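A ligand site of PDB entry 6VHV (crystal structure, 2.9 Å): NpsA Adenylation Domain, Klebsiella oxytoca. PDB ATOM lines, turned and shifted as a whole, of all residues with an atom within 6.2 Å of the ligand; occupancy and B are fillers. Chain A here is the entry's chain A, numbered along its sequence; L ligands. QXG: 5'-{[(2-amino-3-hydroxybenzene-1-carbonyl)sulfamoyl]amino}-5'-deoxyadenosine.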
ATOM      1  N   MET A 160     -12.525  -9.038  -0.341  1.00  0.00           N
ATOM      2  CA  MET A 160     -12.908  -8.659  -1.684  1.00  0.00           C
ATOM      3  C   MET A 160     -11.676  -8.383  -2.542  1.00  0.00           C
ATOM      4  O   MET A 160     -10.604  -8.043  -2.024  1.00  0.00           O
ATOM      5  CB  MET A 160     -13.804  -7.409  -1.666  1.00  0.00           C
ATOM      6  CG  MET A 160     -15.079  -7.584  -0.859  1.00  0.00           C
ATOM      7  SD  MET A 160     -16.256  -8.703  -1.638  1.00  0.00           S
ATOM      8  CE  MET A 160     -17.175  -9.263  -0.216  1.00  0.00           C
ATOM      9  N   THR A 161     -11.833  -8.538  -3.851  1.00  0.00           N
ATOM     10  CA  THR A 161     -10.787  -8.209  -4.800  1.00  0.00           C
ATOM     11  C   THR A 161     -11.427  -7.773  -6.109  1.00  0.00           C
ATOM     12  O   THR A 161     -12.544  -8.195  -6.447  1.00  0.00           O
ATOM     13  CB  THR A 161      -9.843  -9.402  -5.041  1.00  0.00           C
ATOM     14  OG1 THR A 161      -8.859  -9.056  -6.021  1.00  0.00           O
ATOM     15  CG2 THR A 161     -10.609 -10.625  -5.499  1.00  0.00           C
ATOM     16  N   PHE A 204      -8.464  -4.994   3.306  1.00  0.00           N
ATOM     17  CA  PHE A 204      -7.417  -5.407   2.386  1.00  0.00           C
ATOM     18  C   PHE A 204      -6.596  -6.504   3.040  1.00  0.00           C
ATOM     19  O   PHE A 204      -6.221  -6.393   4.208  1.00  0.00           O
ATOM     20  CB  PHE A 204      -6.546  -4.200   2.012  1.00  0.00           C
ATOM     21  CG  PHE A 204      -5.427  -4.516   1.069  1.00  0.00           C
ATOM     22  CD1 PHE A 204      -4.193  -3.899   1.225  1.00  0.00           C
ATOM     23  CD2 PHE A 204      -5.599  -5.408   0.028  1.00  0.00           C
ATOM     24  CE1 PHE A 204      -3.158  -4.175   0.351  1.00  0.00           C
ATOM     25  CE2 PHE A 204      -4.558  -5.688  -0.834  1.00  0.00           C
ATOM     26  CZ  PHE A 204      -3.336  -5.068  -0.671  1.00  0.00           C
ATOM     27  N   ALA A 205      -6.302  -7.564   2.272  1.00  0.00           N
ATOM     28  CA  ALA A 205      -5.706  -8.767   2.844  1.00  0.00           C
ATOM     29  C   ALA A 205      -4.314  -8.535   3.420  1.00  0.00           C
ATOM     30  O   ALA A 205      -3.828  -9.377   4.188  1.00  0.00           O
ATOM     31  CB  ALA A 205      -5.658  -9.868   1.790  1.00  0.00           C
ATOM     32  N   ALA A 206      -3.663  -7.424   3.072  1.00  0.00           N
ATOM     33  CA  ALA A 206      -2.327  -7.164   3.610  1.00  0.00           C
ATOM     34  C   ALA A 206      -2.347  -6.824   5.093  1.00  0.00           C
ATOM     35  O   ALA A 206      -1.306  -6.876   5.746  1.00  0.00           O
ATOM     36  CB  ALA A 206      -1.668  -6.031   2.833  1.00  0.00           C
ATOM     37  N   SER A 207      -3.526  -6.487   5.636  1.00  0.00           N
ATOM     38  CA  SER A 207      -3.615  -6.211   7.071  1.00  0.00           C
ATOM     39  C   SER A 207      -3.478  -7.477   7.907  1.00  0.00           C
ATOM     40  O   SER A 207      -3.189  -7.384   9.109  1.00  0.00           O
ATOM     41  CB  SER A 207      -4.949  -5.526   7.393  1.00  0.00           C
ATOM     42  OG  SER A 207      -6.041  -6.260   6.876  1.00  0.00           O
ATOM     43  N   ASN A 209      -1.081  -9.605   7.528  1.00  0.00           N
ATOM     44  CA  ASN A 209       0.350  -9.693   7.824  1.00  0.00           C
ATOM     45  C   ASN A 209       0.700  -8.991   9.125  1.00  0.00           C
ATOM     46  O   ASN A 209       1.598  -9.427   9.855  1.00  0.00           O
ATOM     47  CB  ASN A 209       1.164  -9.101   6.675  1.00  0.00           C
ATOM     48  CG  ASN A 209       0.665  -9.540   5.308  1.00  0.00           C
ATOM     49  OD1 ASN A 209      -0.015 -10.554   5.188  1.00  0.00           O
ATOM     50  ND2 ASN A 209       1.005  -8.773   4.285  1.00  0.00           N
ATOM     51  N   PHE A 247       5.490  -3.752   7.298  1.00  0.00           N
ATOM     52  CA  PHE A 247       4.892  -4.140   6.028  1.00  0.00           C
ATOM     53  C   PHE A 247       4.405  -2.895   5.305  1.00  0.00           C
ATOM     54  O   PHE A 247       3.572  -2.154   5.841  1.00  0.00           O
ATOM     55  CB  PHE A 247       3.750  -5.128   6.229  1.00  0.00           C
ATOM     56  CG  PHE A 247       4.187  -6.515   6.589  1.00  0.00           C
ATOM     57  CD1 PHE A 247       4.237  -6.919   7.913  1.00  0.00           C
ATOM     58  CD2 PHE A 247       4.554  -7.423   5.612  1.00  0.00           C
ATOM     59  CE1 PHE A 247       4.643  -8.204   8.257  1.00  0.00           C
ATOM     60  CE2 PHE A 247       4.970  -8.698   5.939  1.00  0.00           C
ATOM     61  CZ  PHE A 247       5.005  -9.085   7.259  1.00  0.00           C
ATOM     62  N   LEU A 248       4.922  -2.660   4.109  1.00  0.00           N
ATOM     63  CA  LEU A 248       4.572  -1.486   3.322  1.00  0.00           C
ATOM     64  C   LEU A 248       4.053  -1.895   1.950  1.00  0.00           C
ATOM     65  O   LEU A 248       4.375  -2.969   1.434  1.00  0.00           O
ATOM     66  CB  LEU A 248       5.783  -0.559   3.140  1.00  0.00           C
ATOM     67  CG  LEU A 248       6.438   0.027   4.389  1.00  0.00           C
ATOM     68  CD1 LEU A 248       7.535   1.013   4.003  1.00  0.00           C
ATOM     69  CD2 LEU A 248       5.389   0.698   5.270  1.00  0.00           C
ATOM     70  N   VAL A 272       8.168  -4.984   1.267  1.00  0.00           N
ATOM     71  CA  VAL A 272       7.429  -4.269   0.226  1.00  0.00           C
ATOM     72  C   VAL A 272       6.632  -5.286  -0.578  1.00  0.00           C
ATOM     73  O   VAL A 272       7.180  -6.292  -1.035  1.00  0.00           O
ATOM     74  CB  VAL A 272       8.378  -3.478  -0.686  1.00  0.00           C
ATOM     75  CG1 VAL A 272       7.587  -2.551  -1.593  1.00  0.00           C
ATOM     76  CG2 VAL A 272       9.384  -2.695   0.143  1.00  0.00           C
ATOM     77  N   SER A 273       5.337  -5.024  -0.744  1.00  0.00           N
ATOM     78  CA  SER A 273       4.455  -5.986  -1.383  1.00  0.00           C
ATOM     79  C   SER A 273       3.279  -5.259  -2.020  1.00  0.00           C
ATOM     80  O   SER A 273       2.950  -4.122  -1.651  1.00  0.00           O
ATOM     81  CB  SER A 273       3.954  -7.044  -0.390  1.00  0.00           C
ATOM     82  OG  SER A 273       3.300  -6.430   0.706  1.00  0.00           O
ATOM     83  N   GLY A 274       2.646  -5.929  -2.981  1.00  0.00           N
ATOM     84  CA  GLY A 274       1.404  -5.478  -3.572  1.00  0.00           C
ATOM     85  C   GLY A 274       1.500  -5.102  -5.039  1.00  0.00           C
ATOM     86  O   GLY A 274       0.505  -5.227  -5.761  1.00  0.00           O
ATOM     87  N   ASP A 275       2.665  -4.670  -5.499  1.00  0.00           N
ATOM     88  CA  ASP A 275       2.770  -4.135  -6.847  1.00  0.00           C
ATOM     89  C   ASP A 275       4.241  -4.108  -7.249  1.00  0.00           C
ATOM     90  O   ASP A 275       5.139  -4.268  -6.429  1.00  0.00           O
ATOM     91  CB  ASP A 275       2.151  -2.741  -6.940  1.00  0.00           C
ATOM     92  CG  ASP A 275       1.809  -2.342  -8.351  1.00  0.00           C
ATOM     93  OD1 ASP A 275       2.069  -3.145  -9.274  1.00  0.00           O
ATOM     94  OD2 ASP A 275       1.273  -1.221  -8.538  1.00  0.00           O
ATOM     95  N   PHE A 276       4.459  -3.906  -8.548  1.00  0.00           N
ATOM     96  CA  PHE A 276       5.810  -3.707  -9.054  1.00  0.00           C
ATOM     97  C   PHE A 276       6.324  -2.331  -8.630  1.00  0.00           C
ATOM     98  O   PHE A 276       5.570  -1.368  -8.519  1.00  0.00           O
ATOM     99  CB  PHE A 276       5.838  -3.825 -10.584  1.00  0.00           C
ATOM    100  CG  PHE A 276       5.560  -5.209 -11.088  1.00  0.00           C
ATOM    101  CD1 PHE A 276       4.298  -5.555 -11.544  1.00  0.00           C
ATOM    102  CD2 PHE A 276       6.556  -6.179 -11.118  1.00  0.00           C
ATOM    103  CE1 PHE A 276       4.033  -6.831 -12.016  1.00  0.00           C
ATOM    104  CE2 PHE A 276       6.296  -7.446 -11.588  1.00  0.00           C
ATOM    105  CZ  PHE A 276       5.037  -7.774 -12.031  1.00  0.00           C
ATOM    106  N   VAL A 277       7.640  -2.256  -8.394  1.00  0.00           N
ATOM    107  CA  VAL A 277       8.281  -1.051  -7.885  1.00  0.00           C
ATOM    108  C   VAL A 277       9.593  -0.858  -8.637  1.00  0.00           C
ATOM    109  O   VAL A 277      10.267  -1.833  -8.986  1.00  0.00           O
ATOM    110  CB  VAL A 277       8.502  -1.145  -6.358  1.00  0.00           C
ATOM    111  CG1 VAL A 277       9.425  -0.039  -5.875  1.00  0.00           C
ATOM    112  CG2 VAL A 277       7.175  -1.092  -5.617  1.00  0.00           C
ATOM    113  N   ASN A 295      11.292  -7.822  -1.014  1.00  0.00           N
ATOM    114  CA  ASN A 295      10.174  -7.799  -1.937  1.00  0.00           C
ATOM    115  C   ASN A 295       9.405  -9.104  -1.767  1.00  0.00           C
ATOM    116  O   ASN A 295       9.999 -10.174  -1.621  1.00  0.00           O
ATOM    117  CB  ASN A 295      10.643  -7.651  -3.388  1.00  0.00           C
ATOM    118  CG  ASN A 295       9.490  -7.563  -4.362  1.00  0.00           C
ATOM    119  OD1 ASN A 295       8.444  -6.982  -4.055  1.00  0.00           O
ATOM    120  ND2 ASN A 295       9.660  -8.154  -5.545  1.00  0.00           N
ATOM    121  N   GLY A 296       8.072  -9.006  -1.786  1.00  0.00           N
ATOM    122  CA  GLY A 296       7.256 -10.170  -1.528  1.00  0.00           C
ATOM    123  C   GLY A 296       5.967 -10.162  -2.320  1.00  0.00           C
ATOM    124  O   GLY A 296       5.518  -9.119  -2.789  1.00  0.00           O
ATOM    125  N   LEU A 297       5.388 -11.350  -2.459  1.00  0.00           N
ATOM    126  CA  LEU A 297       4.125 -11.523  -3.148  1.00  0.00           C
ATOM    127  C   LEU A 297       3.024 -11.769  -2.127  1.00  0.00           C
ATOM    128  O   LEU A 297       3.111 -12.689  -1.308  1.00  0.00           O
ATOM    129  CB  LEU A 297       4.169 -12.689  -4.133  1.00  0.00           C
ATOM    130  CG  LEU A 297       2.794 -13.023  -4.721  1.00  0.00           C
ATOM    131  CD1 LEU A 297       2.521 -12.224  -5.980  1.00  0.00           C
ATOM    132  CD2 LEU A 297       2.628 -14.517  -4.972  1.00  0.00           C
ATOM    133  N   GLY A 298       1.993 -10.926  -2.159  1.00  0.00           N
ATOM    134  CA  GLY A 298       0.785 -11.151  -1.385  1.00  0.00           C
ATOM    135  C   GLY A 298      -0.385 -11.344  -2.328  1.00  0.00           C
ATOM    136  O   GLY A 298      -0.473 -10.687  -3.364  1.00  0.00           O
ATOM    137  N   CYS A 299      -1.284 -12.249  -1.955  1.00  0.00           N
ATOM    138  CA  CYS A 299      -2.426 -12.590  -2.793  1.00  0.00           C
ATOM    139  C   CYS A 299      -3.654 -12.762  -1.916  1.00  0.00           C
ATOM    140  O   CYS A 299      -3.590 -13.461  -0.901  1.00  0.00           O
ATOM    141  CB  CYS A 299      -2.152 -13.876  -3.592  1.00  0.00           C
ATOM    142  SG  CYS A 299      -3.053 -13.990  -5.148  1.00  0.00           S
ATOM    143  N   THR A 300      -4.763 -12.126  -2.314  1.00  0.00           N
ATOM    144  CA  THR A 300      -5.997 -12.255  -1.542  1.00  0.00           C
ATOM    145  C   THR A 300      -6.434 -13.712  -1.449  1.00  0.00           C
ATOM    146  O   THR A 300      -6.813 -14.191  -0.380  1.00  0.00           O
ATOM    147  CB  THR A 300      -7.104 -11.405  -2.159  1.00  0.00           C
ATOM    148  OG1 THR A 300      -6.717 -10.023  -2.157  1.00  0.00           O
ATOM    149  CG2 THR A 300      -8.393 -11.548  -1.375  1.00  0.00           C
ATOM    150  N   GLU A 301      -6.374 -14.436  -2.572  1.00  0.00           N
ATOM    151  CA  GLU A 301      -6.800 -15.821  -2.597  1.00  0.00           C
ATOM    152  C   GLU A 301      -5.858 -16.752  -1.851  1.00  0.00           C
ATOM    153  O   GLU A 301      -6.179 -17.931  -1.681  1.00  0.00           O
ATOM    154  CB  GLU A 301      -6.964 -16.281  -4.054  1.00  0.00           C
ATOM    155  CG  GLU A 301      -8.105 -15.602  -4.798  1.00  0.00           C
ATOM    156  CD  GLU A 301      -7.717 -14.268  -5.412  1.00  0.00           C
ATOM    157  OE1 GLU A 301      -6.750 -13.644  -4.933  1.00  0.00           O
ATOM    158  OE2 GLU A 301      -8.390 -13.850  -6.384  1.00  0.00           O
ATOM    159  N   SER A 303      -4.804 -15.660   1.253  1.00  0.00           N
ATOM    160  CA  SER A 303      -5.030 -15.178   2.611  1.00  0.00           C
ATOM    161  C   SER A 303      -4.142 -14.001   3.012  1.00  0.00           C
ATOM    162  O   SER A 303      -4.639 -13.000   3.518  1.00  0.00           O
ATOM    163  CB  SER A 303      -4.872 -16.321   3.621  1.00  0.00           C
ATOM    164  OG  SER A 303      -5.801 -17.358   3.363  1.00  0.00           O
ATOM    165  N   ALA A 304      -2.831 -14.116   2.822  1.00  0.00           N
ATOM    166  CA  ALA A 304      -1.939 -13.082   3.343  1.00  0.00           C
ATOM    167  C   ALA A 304      -0.639 -13.090   2.533  1.00  0.00           C
ATOM    168  O   ALA A 304      -0.606 -13.574   1.394  1.00  0.00           O
ATOM    169  CB  ALA A 304      -1.699 -13.308   4.847  1.00  0.00           C
ATOM    170  N   ILE A 305       0.426 -12.532   3.114  1.00  0.00           N
ATOM    171  CA  ILE A 305       1.730 -12.540   2.474  1.00  0.00           C
ATOM    172  C   ILE A 305       2.162 -13.971   2.206  1.00  0.00           C
ATOM    173  O   ILE A 305       1.891 -14.872   3.001  1.00  0.00           O
ATOM    174  CB  ILE A 305       2.747 -11.779   3.347  1.00  0.00           C
ATOM    175  CG1 ILE A 305       4.118 -11.708   2.671  1.00  0.00           C
ATOM    176  CG2 ILE A 305       2.851 -12.409   4.729  1.00  0.00           C
ATOM    177  CD1 ILE A 305       4.160 -10.797   1.462  1.00  0.00           C
ATOM    178  N   SER A 306       2.817 -14.188   1.071  1.00  0.00           N
ATOM    179  CA  SER A 306       3.047 -15.551   0.601  1.00  0.00           C
ATOM    180  C   SER A 306       4.521 -15.865   0.338  1.00  0.00           C
ATOM    181  O   SER A 306       4.963 -17.000   0.556  1.00  0.00           O
ATOM    182  CB  SER A 306       2.225 -15.815  -0.652  1.00  0.00           C
ATOM    183  OG  SER A 306       0.849 -15.600  -0.404  1.00  0.00           O
ATOM    184  N   VAL A 323      12.586  -7.197  -9.861  1.00  0.00           N
ATOM    185  CA  VAL A 323      13.064  -7.829  -8.629  1.00  0.00           C
ATOM    186  C   VAL A 323      12.217  -9.073  -8.344  1.00  0.00           C
ATOM    187  O   VAL A 323      10.984  -9.021  -8.491  1.00  0.00           O
ATOM    188  CB  VAL A 323      12.991  -6.838  -7.463  1.00  0.00           C
ATOM    189  CG1 VAL A 323      13.542  -7.452  -6.184  1.00  0.00           C
ATOM    190  CG2 VAL A 323      13.756  -5.564  -7.806  1.00  0.00           C
ATOM    191  N   PRO A 324      12.829 -10.193  -7.962  1.00  0.00           N
ATOM    192  CA  PRO A 324      12.041 -11.404  -7.676  1.00  0.00           C
ATOM    193  C   PRO A 324      11.159 -11.227  -6.451  1.00  0.00           C
ATOM    194  O   PRO A 324      11.332 -10.315  -5.641  1.00  0.00           O
ATOM    195  CB  PRO A 324      13.113 -12.474  -7.433  1.00  0.00           C
ATOM    196  CG  PRO A 324      14.346 -11.936  -8.075  1.00  0.00           C
ATOM    197  CD  PRO A 324      14.278 -10.447  -7.913  1.00  0.00           C
ATOM    198  N   VAL A 325      10.185 -12.145  -6.327  1.00  0.00           N
ATOM    199  CA  VAL A 325       9.361 -12.223  -5.129  1.00  0.00           C
ATOM    200  C   VAL A 325       9.806 -13.330  -4.190  1.00  0.00           C
ATOM    201  O   VAL A 325       9.250 -13.458  -3.085  1.00  0.00           O
ATOM    202  CB  VAL A 325       7.863 -12.404  -5.474  1.00  0.00           C
ATOM    203  CG1 VAL A 325       7.354 -11.204  -6.260  1.00  0.00           C
ATOM    204  CG2 VAL A 325       7.651 -13.698  -6.247  1.00  0.00           C
ATOM    205  N   TYR A 386      -4.296 -22.745  -6.589  1.00  0.00           N
ATOM    206  CA  TYR A 386      -4.982 -21.557  -7.076  1.00  0.00           C
ATOM    207  C   TYR A 386      -4.155 -20.933  -8.187  1.00  0.00           C
ATOM    208  O   TYR A 386      -2.932 -20.822  -8.075  1.00  0.00           O
ATOM    209  CB  TYR A 386      -5.205 -20.546  -5.948  1.00  0.00           C
ATOM    210  CG  TYR A 386      -5.439 -19.132  -6.449  1.00  0.00           C
ATOM    211  CD1 TYR A 386      -6.669 -18.750  -6.988  1.00  0.00           C
ATOM    212  CD2 TYR A 386      -4.438 -18.173  -6.383  1.00  0.00           C
ATOM    213  CE1 TYR A 386      -6.884 -17.470  -7.448  1.00  0.00           C
ATOM    214  CE2 TYR A 386      -4.649 -16.885  -6.841  1.00  0.00           C
ATOM    215  CZ  TYR A 386      -5.875 -16.538  -7.370  1.00  0.00           C
ATOM    216  OH  TYR A 386      -6.077 -15.253  -7.826  1.00  0.00           O
ATOM    217  N   THR A 388      -3.004 -17.785 -10.252  1.00  0.00           N
ATOM    218  CA  THR A 388      -2.882 -16.352 -10.051  1.00  0.00           C
ATOM    219  C   THR A 388      -3.161 -15.531 -11.300  1.00  0.00           C
ATOM    220  O   THR A 388      -3.478 -14.341 -11.187  1.00  0.00           O
ATOM    221  CB  THR A 388      -1.472 -16.003  -9.556  1.00  0.00           C
ATOM    222  OG1 THR A 388      -0.532 -16.242 -10.618  1.00  0.00           O
ATOM    223  CG2 THR A 388      -1.097 -16.841  -8.350  1.00  0.00           C
ATOM    224  N   ASP A 389      -3.051 -16.132 -12.483  1.00  0.00           N
ATOM    225  CA  ASP A 389      -3.035 -15.397 -13.744  1.00  0.00           C
ATOM    226  C   ASP A 389      -1.956 -14.314 -13.686  1.00  0.00           C
ATOM    227  O   ASP A 389      -2.153 -13.160 -14.084  1.00  0.00           O
ATOM    228  CB  ASP A 389      -4.423 -14.824 -14.059  1.00  0.00           C
ATOM    229  CG  ASP A 389      -4.475 -14.074 -15.374  1.00  0.00           C
ATOM    230  OD1 ASP A 389      -4.765 -12.857 -15.345  1.00  0.00           O
ATOM    231  OD2 ASP A 389      -4.180 -14.681 -16.431  1.00  0.00           O
ATOM    232  N   ASP A 390      -0.801 -14.689 -13.151  1.00  0.00           N
ATOM    233  CA  ASP A 390       0.423 -13.897 -13.157  1.00  0.00           C
ATOM    234  C   ASP A 390       1.448 -14.671 -13.958  1.00  0.00           C
ATOM    235  O   ASP A 390       1.847 -15.771 -13.552  1.00  0.00           O
ATOM    236  CB  ASP A 390       0.951 -13.650 -11.749  1.00  0.00           C
ATOM    237  CG  ASP A 390       0.211 -12.548 -11.013  1.00  0.00           C
ATOM    238  OD1 ASP A 390       0.404 -11.366 -11.352  1.00  0.00           O
ATOM    239  OD2 ASP A 390      -0.545 -12.872 -10.082  1.00  0.00           O
ATOM    240  N   LEU A 402       7.978 -12.302 -11.061  1.00  0.00           N
ATOM    241  CA  LEU A 402       6.783 -11.937 -11.811  1.00  0.00           C
ATOM    242  C   LEU A 402       7.148 -11.074 -12.999  1.00  0.00           C
ATOM    243  O   LEU A 402       8.114 -10.301 -12.966  1.00  0.00           O
ATOM    244  CB  LEU A 402       5.791 -11.195 -10.906  1.00  0.00           C
ATOM    245  CG  LEU A 402       5.463 -11.862  -9.566  1.00  0.00           C
ATOM    246  CD1 LEU A 402       4.484 -10.994  -8.786  1.00  0.00           C
ATOM    247  CD2 LEU A 402       4.908 -13.253  -9.772  1.00  0.00           C
ATOM    248  N   GLY A 404       4.202 -10.437 -15.568  1.00  0.00           N
ATOM    249  CA  GLY A 404       2.961  -9.978 -16.147  1.00  0.00           C
ATOM    250  C   GLY A 404       1.757 -10.367 -15.318  1.00  0.00           C
ATOM    251  O   GLY A 404       1.878 -10.848 -14.186  1.00  0.00           O
ATOM    252  N   ARG A 405       0.570 -10.154 -15.905  1.00  0.00           N
ATOM    253  CA  ARG A 405      -0.666 -10.434 -15.185  1.00  0.00           C
ATOM    254  C   ARG A 405      -1.815 -10.869 -16.094  1.00  0.00           C
ATOM    255  O   ARG A 405      -2.973 -10.846 -15.647  1.00  0.00           O
ATOM    256  CB  ARG A 405      -1.118  -9.191 -14.385  1.00  0.00           C
ATOM    257  N   LYS A 494      -0.758   1.130  -4.472  1.00  0.00           N
ATOM    258  CA  LYS A 494      -0.358   0.639  -5.783  1.00  0.00           C
ATOM    259  C   LYS A 494      -0.951   1.495  -6.882  1.00  0.00           C
ATOM    260  O   LYS A 494      -1.942   2.196  -6.697  1.00  0.00           O
ATOM    261  CB  LYS A 494      -0.774  -0.830  -5.959  1.00  0.00           C
ATOM    262  CG  LYS A 494      -2.237  -1.095  -5.694  1.00  0.00           C
ATOM    263  CD  LYS A 494      -2.560  -2.570  -5.850  1.00  0.00           C
ATOM    264  CE  LYS A 494      -1.874  -3.390  -4.781  1.00  0.00           C
ATOM    265  NZ  LYS A 494      -2.160  -4.843  -4.954  1.00  0.00           N
HETATM  266  N10 QXG L   1       1.299  -8.301  -6.947  1.00  0.00           N
HETATM  267  C02 QXG L   1       4.840  -7.781  -6.265  1.00  0.00           C
HETATM  268  C04 QXG L   1       4.400  -7.151  -8.499  1.00  0.00           C
HETATM  269  C06 QXG L   1       2.609  -7.908  -7.308  1.00  0.00           C
HETATM  270  C07 QXG L   1       3.422  -8.108  -6.159  1.00  0.00           C
HETATM  271  C09 QXG L   1       1.350  -8.733  -5.593  1.00  0.00           C
HETATM  272  C11 QXG L   1       0.091  -8.299  -7.754  1.00  0.00           C
HETATM  273  C13 QXG L   1      -1.933  -9.298  -7.131  1.00  0.00           C
HETATM  274  C14 QXG L   1      -2.747  -9.674  -5.864  1.00  0.00           C
HETATM  275  C20 QXG L   1      -2.615  -8.474  -2.081  1.00  0.00           C
HETATM  276  C22 QXG L   1      -1.846  -8.803  -0.785  1.00  0.00           C
HETATM  277  C23 QXG L   1      -2.402  -9.761   0.122  1.00  0.00           C
HETATM  278  C24 QXG L   1      -1.765 -10.108   1.308  1.00  0.00           C
HETATM  279  C25 QXG L   1      -0.527  -9.491   1.635  1.00  0.00           C
HETATM  280  C26 QXG L   1       0.024  -8.557   0.745  1.00  0.00           C
HETATM  281  C28 QXG L   1      -0.592  -8.166  -0.484  1.00  0.00           C
HETATM  282  C30 QXG L   1      -0.960 -10.400  -7.632  1.00  0.00           C
HETATM  283  C32 QXG L   1      -0.012  -9.659  -8.568  1.00  0.00           C
HETATM  284  N01 QXG L   1       5.748  -7.920  -5.228  1.00  0.00           N
HETATM  285  N03 QXG L   1       5.302  -7.300  -7.454  1.00  0.00           N
HETATM  286  N05 QXG L   1       3.074  -7.427  -8.507  1.00  0.00           N
HETATM  287  N08 QXG L   1       2.611  -8.616  -5.120  1.00  0.00           N
HETATM  288  N15 QXG L   1      -3.435  -8.505  -5.243  1.00  0.00           N
HETATM  289  N19 QXG L   1      -3.869  -9.034  -2.568  1.00  0.00           N
HETATM  290  N29 QXG L   1      -0.013  -7.226  -1.343  1.00  0.00           N
HETATM  291  O12 QXG L   1      -1.010  -8.221  -6.905  1.00  0.00           O
HETATM  292  O17 QXG L   1      -5.611  -9.537  -4.430  1.00  0.00           O
HETATM  293  O18 QXG L   1      -5.205  -7.287  -3.947  1.00  0.00           O
HETATM  294  O21 QXG L   1      -2.146  -7.646  -2.814  1.00  0.00           O
HETATM  295  O27 QXG L   1       1.224  -7.937   1.017  1.00  0.00           O
HETATM  296  O31 QXG L   1      -1.593 -11.450  -8.351  1.00  0.00           O
HETATM  297  O33 QXG L   1      -0.626  -9.474  -9.799  1.00  0.00           O
HETATM  298  S16 QXG L   1      -4.644  -8.577  -4.069  1.00  0.00           S
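O of Asp 275 sits close to N03 of the ligand.
Merely in contact with the ligand: Phe 276, Gly 298, Ala 304, Cys 299, Ile 305, Lys 494, Ala 206, Phe 204, Ala 205, Thr 161, Leu 297, Val 325 and Leu 402.
Hydrophobic or aromatic side chains within 4 Å of the ligand: Phe 204, Ala 205, Ala 206, Phe 276, Leu 297, Val 325 and Leu 402.
Within 4 Å of the ligand: Thr 161, Phe 204, Ala 205, Ala 206, Asn 209, Ser 273, Gly 274, Asp 275, Phe 276, Asn 295, Gly 296, Leu 297, Gly 298, Cys 299, Thr 300, Ala 304, Ile 305, Val 325, Asp 390, Leu 402 and Lys 494.
The nearest printed residue that does not touch the ligand is Glu 301 (4.3 Å).
The side-chain hydroxyl (OG) of Ser 273 is in hydrogen-bond range of an oxygen (O27) of the ligand (2.6 Å).
The side-chain amide nitrogen (ND2) of Asn 209 lies close to an oxygen (O27) of the ligand, 3.4 Å away.
The side-chain amide oxygen (OD1) of Asn 295 sits at hydrogen-bond distance from a nitrogen (N01) of the ligand, at 3.1 Å.
N19 of the ligand lies within hydrogen-bond range of N of Thr 300 (3.2 Å).
OD2 of Asp 390 sits at hydrogen-bond distance from O31 of the ligand.
The backbone carbonyl oxygen (O) of Gly 296 lies within hydrogen-bond range of a nitrogen (N01) of the ligand, 2.7 Å away.
OG1 of Thr 300 is in hydrogen-bond range of O17 of the ligand (2.6 Å).
The backbone NH of Gly 274 is in hydrogen-bond range of a nitrogen (N08) of the ligand (3.4 Å).
ND2 of Asn 295 lies within hydrogen-bond range of O of Val 323, at 3.3 Å.
ND2 of Asn 295 lies within hydrogen-bond range of O of Pro 324, at 2.7 Å.
The side-chain amide nitrogen (ND2) of Asn 209 sits at hydrogen-bond distance from the backbone carbonyl oxygen (O) of Ala 206, at 3.3 Å.
OD1 of Asn 209 sits at hydrogen-bond distance from N of Ile 305, 2.9 Å away.
The side-chain sulfur (SG) of Cys 299 is in hydrogen-bond range of the side-chain carboxylate (OE1) of Glu 301.
OD1 of Asn 295 sits close to O of Val 272 (3.3 Å).
The backbone carbonyl oxygen of Leu 297 lies within hydrogen-bond range of the backbone NH of Ser 306 (2.8 Å).
N of Ser 273 is in hydrogen-bond range of O of Leu 248.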
